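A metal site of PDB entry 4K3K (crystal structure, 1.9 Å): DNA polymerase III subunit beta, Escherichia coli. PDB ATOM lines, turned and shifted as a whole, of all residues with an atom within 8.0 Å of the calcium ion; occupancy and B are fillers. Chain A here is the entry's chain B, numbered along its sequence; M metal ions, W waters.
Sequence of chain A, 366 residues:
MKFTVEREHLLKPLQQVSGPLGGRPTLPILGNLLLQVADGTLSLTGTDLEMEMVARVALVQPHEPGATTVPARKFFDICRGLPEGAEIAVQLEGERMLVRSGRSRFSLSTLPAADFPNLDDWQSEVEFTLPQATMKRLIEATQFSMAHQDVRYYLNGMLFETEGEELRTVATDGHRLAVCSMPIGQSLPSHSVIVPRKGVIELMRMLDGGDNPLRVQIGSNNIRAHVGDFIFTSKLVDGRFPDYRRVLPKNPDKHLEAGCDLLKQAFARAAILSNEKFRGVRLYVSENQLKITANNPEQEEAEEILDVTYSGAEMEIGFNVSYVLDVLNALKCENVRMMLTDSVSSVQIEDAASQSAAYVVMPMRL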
ATOM      1  N   VAL A   5      11.613 -21.404 -16.276  1.00  0.00           N
ATOM      2  CA  VAL A   5      12.839 -20.649 -16.018  1.00  0.00           C
ATOM      3  C   VAL A   5      14.006 -21.611 -15.868  1.00  0.00           C
ATOM      4  O   VAL A   5      13.858 -22.687 -15.289  1.00  0.00           O
ATOM      5  CB  VAL A   5      12.691 -19.766 -14.756  1.00  0.00           C
ATOM      6  CG1 VAL A   5      14.015 -19.099 -14.371  1.00  0.00           C
ATOM      7  CG2 VAL A   5      11.616 -18.727 -14.962  1.00  0.00           C
ATOM      8  N   GLU A   6      15.171 -21.238 -16.404  1.00  0.00           N
ATOM      9  CA  GLU A   6      16.351 -22.053 -16.211  1.00  0.00           C
ATOM     10  C   GLU A   6      16.788 -22.023 -14.743  1.00  0.00           C
ATOM     11  O   GLU A   6      16.697 -20.988 -14.080  1.00  0.00           O
ATOM     12  CB  GLU A   6      17.509 -21.634 -17.121  1.00  0.00           C
ATOM     13  CG  GLU A   6      18.568 -22.702 -17.222  1.00  0.00           C
ATOM     14  CD  GLU A   6      19.594 -22.432 -18.301  1.00  0.00           C
ATOM     15  OE1 GLU A   6      20.125 -21.304 -18.307  1.00  0.00           O
ATOM     16  OE2 GLU A   6      19.864 -23.340 -19.119  1.00  0.00           O
ATOM     17  N   ARG A   7      17.243 -23.168 -14.260  1.00  0.00           N
ATOM     18  CA  ARG A   7      17.561 -23.391 -12.845  1.00  0.00           C
ATOM     19  C   ARG A   7      18.324 -22.263 -12.166  1.00  0.00           C
ATOM     20  O   ARG A   7      17.894 -21.745 -11.126  1.00  0.00           O
ATOM     21  CB  ARG A   7      18.387 -24.679 -12.727  1.00  0.00           C
ATOM     22  CG  ARG A   7      18.913 -24.985 -11.342  1.00  0.00           C
ATOM     23  CD  ARG A   7      19.536 -26.360 -11.315  1.00  0.00           C
ATOM     24  NE  ARG A   7      20.225 -26.651 -10.064  1.00  0.00           N
ATOM     25  CZ  ARG A   7      21.493 -26.328  -9.797  1.00  0.00           C
ATOM     26  NH1 ARG A   7      22.241 -25.678 -10.680  1.00  0.00           N
ATOM     27  NH2 ARG A   7      22.019 -26.665  -8.626  1.00  0.00           N
ATOM     28  N   GLU A   8      19.443 -21.876 -12.761  1.00  0.00           N
ATOM     29  CA  GLU A   8      20.367 -20.943 -12.112  1.00  0.00           C
ATOM     30  C   GLU A   8      19.834 -19.516 -12.025  1.00  0.00           C
ATOM     31  O   GLU A   8      20.331 -18.718 -11.240  1.00  0.00           O
ATOM     32  CB  GLU A   8      21.742 -20.966 -12.792  1.00  0.00           C
ATOM     33  CG  GLU A   8      22.451 -22.319 -12.718  1.00  0.00           C
ATOM     34  CD  GLU A   8      21.817 -23.370 -13.607  1.00  0.00           C
ATOM     35  OE1 GLU A   8      21.307 -23.035 -14.699  1.00  0.00           O
ATOM     36  OE2 GLU A   8      21.824 -24.558 -13.225  1.00  0.00           O
ATOM     37  N   GLN A  61      11.047 -16.913 -21.371  1.00  0.00           N
ATOM     38  CA  GLN A  61      10.320 -18.048 -21.957  1.00  0.00           C
ATOM     39  C   GLN A  61       8.830 -17.807 -21.810  1.00  0.00           C
ATOM     40  O   GLN A  61       8.406 -16.987 -20.997  1.00  0.00           O
ATOM     41  CB  GLN A  61      10.726 -19.375 -21.279  1.00  0.00           C
ATOM     42  CG  GLN A  61      12.220 -19.608 -21.206  1.00  0.00           C
ATOM     43  CD  GLN A  61      12.592 -21.045 -20.868  1.00  0.00           C
ATOM     44  OE1 GLN A  61      12.021 -21.992 -21.430  1.00  0.00           O
ATOM     45  NE2 GLN A  61      13.534 -21.223 -19.946  1.00  0.00           N
ATOM     46  N   PRO A  83      19.465 -30.958 -12.314  1.00  0.00           N
ATOM     47  CA  PRO A  83      20.776 -30.804 -12.925  1.00  0.00           C
ATOM     48  C   PRO A  83      21.031 -29.393 -13.426  1.00  0.00           C
ATOM     49  O   PRO A  83      20.089 -28.623 -13.660  1.00  0.00           O
ATOM     50  CB  PRO A  83      20.757 -31.813 -14.088  1.00  0.00           C
ATOM     51  CG  PRO A  83      19.317 -32.038 -14.372  1.00  0.00           C
ATOM     52  CD  PRO A  83      18.607 -31.886 -13.059  1.00  0.00           C
ATOM     53  N   GLU A  84      22.305 -29.062 -13.555  1.00  0.00           N
ATOM     54  CA  GLU A  84      22.720 -27.739 -13.953  1.00  0.00           C
ATOM     55  C   GLU A  84      22.181 -27.401 -15.337  1.00  0.00           C
ATOM     56  O   GLU A  84      22.322 -28.177 -16.290  1.00  0.00           O
ATOM     57  CB  GLU A  84      24.239 -27.655 -13.934  1.00  0.00           C
ATOM     58  CG  GLU A  84      24.796 -26.295 -14.281  1.00  0.00           C
ATOM     59  CD  GLU A  84      26.235 -26.137 -13.844  1.00  0.00           C
ATOM     60  OE1 GLU A  84      26.950 -27.157 -13.782  1.00  0.00           O
ATOM     61  OE2 GLU A  84      26.634 -24.997 -13.543  1.00  0.00           O
ATOM     62  N   GLY A  85      21.541 -26.244 -15.439  1.00  0.00           N
ATOM     63  CA  GLY A  85      20.918 -25.801 -16.673  1.00  0.00           C
ATOM     64  C   GLY A  85      19.553 -26.407 -16.944  1.00  0.00           C
ATOM     65  O   GLY A  85      18.997 -26.222 -18.017  1.00  0.00           O
ATOM     66  N   ALA A  86      18.983 -27.111 -15.963  1.00  0.00           N
ATOM     67  CA  ALA A  86      17.651 -27.689 -16.104  1.00  0.00           C
ATOM     68  C   ALA A  86      16.609 -26.598 -16.334  1.00  0.00           C
ATOM     69  O   ALA A  86      16.661 -25.528 -15.699  1.00  0.00           O
ATOM     70  CB  ALA A  86      17.297 -28.488 -14.862  1.00  0.00           C
ATOM     71  N   GLU A  87      15.665 -26.864 -17.242  1.00  0.00           N
ATOM     72  CA  GLU A  87      14.535 -25.972 -17.458  1.00  0.00           C
ATOM     73  C   GLU A  87      13.423 -26.367 -16.509  1.00  0.00           C
ATOM     74  O   GLU A  87      12.953 -27.501 -16.522  1.00  0.00           O
ATOM     75  CB  GLU A  87      14.030 -26.067 -18.897  1.00  0.00           C
ATOM     76  CG  GLU A  87      15.092 -25.772 -19.923  1.00  0.00           C
ATOM     77  CD  GLU A  87      15.695 -24.395 -19.757  1.00  0.00           C
ATOM     78  OE1 GLU A  87      14.992 -23.466 -19.313  1.00  0.00           O
ATOM     79  OE2 GLU A  87      16.902 -24.248 -20.076  1.00  0.00           O
ATOM     80  N   ILE A  88      13.026 -25.424 -15.660  1.00  0.00           N
ATOM     81  CA  ILE A  88      12.047 -25.674 -14.620  1.00  0.00           C
ATOM     82  C   ILE A  88      10.708 -25.092 -15.037  1.00  0.00           C
ATOM     83  O   ILE A  88      10.495 -23.883 -14.975  1.00  0.00           O
ATOM     84  CB  ILE A  88      12.526 -25.087 -13.271  1.00  0.00           C
ATOM     85  CG1 ILE A  88      13.953 -25.573 -12.965  1.00  0.00           C
ATOM     86  CG2 ILE A  88      11.554 -25.467 -12.145  1.00  0.00           C
ATOM     87  CD1 ILE A  88      14.445 -25.320 -11.555  1.00  0.00           C
ATOM     88  N   SER A 101      10.717 -30.992 -15.004  1.00  0.00           N
ATOM     89  CA  SER A 101      11.987 -30.760 -15.663  1.00  0.00           C
ATOM     90  C   SER A 101      12.541 -32.105 -16.092  1.00  0.00           C
ATOM     91  O   SER A 101      12.670 -33.012 -15.279  1.00  0.00           O
ATOM     92  CB  SER A 101      12.967 -30.068 -14.718  1.00  0.00           C
ATOM     93  OG  SER A 101      14.146 -29.703 -15.425  1.00  0.00           O
HETATM   94 CA    CA M   1      18.906 -25.393 -20.108  1.00  0.00          CA
HETATM   95  O   HOH W   1      18.139 -27.547 -20.759  1.00  0.00           O
HETATM   96  O   HOH W   2      21.121 -26.049 -20.510  1.00  0.00           O
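The calcium ion is bound by the backbone carbonyl oxygen (O) of Gly 85, the side-chain carboxylate (OE2) of Glu 87, water W2, water W1 and the side-chain carboxylate (OE2) of Glu 6.
Of the 12 residues printed, 3 come within 4 Å of the calcium ion. The nearest printed residue that does not touch the calcium ion is Ala 86 (4.5 Å).
The side-chain carboxylate (OE1) of Glu 87 is in hydrogen-bond range of the side-chain amide nitrogen (NE2) of Gln 61, at 2.7 Å. N of Gly 85 is in hydrogen-bond range of OE2 of Glu 8, 2.8 Å away. OG of Ser 101 lies within hydrogen-bond range of O of Glu 87 (2.7 Å).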
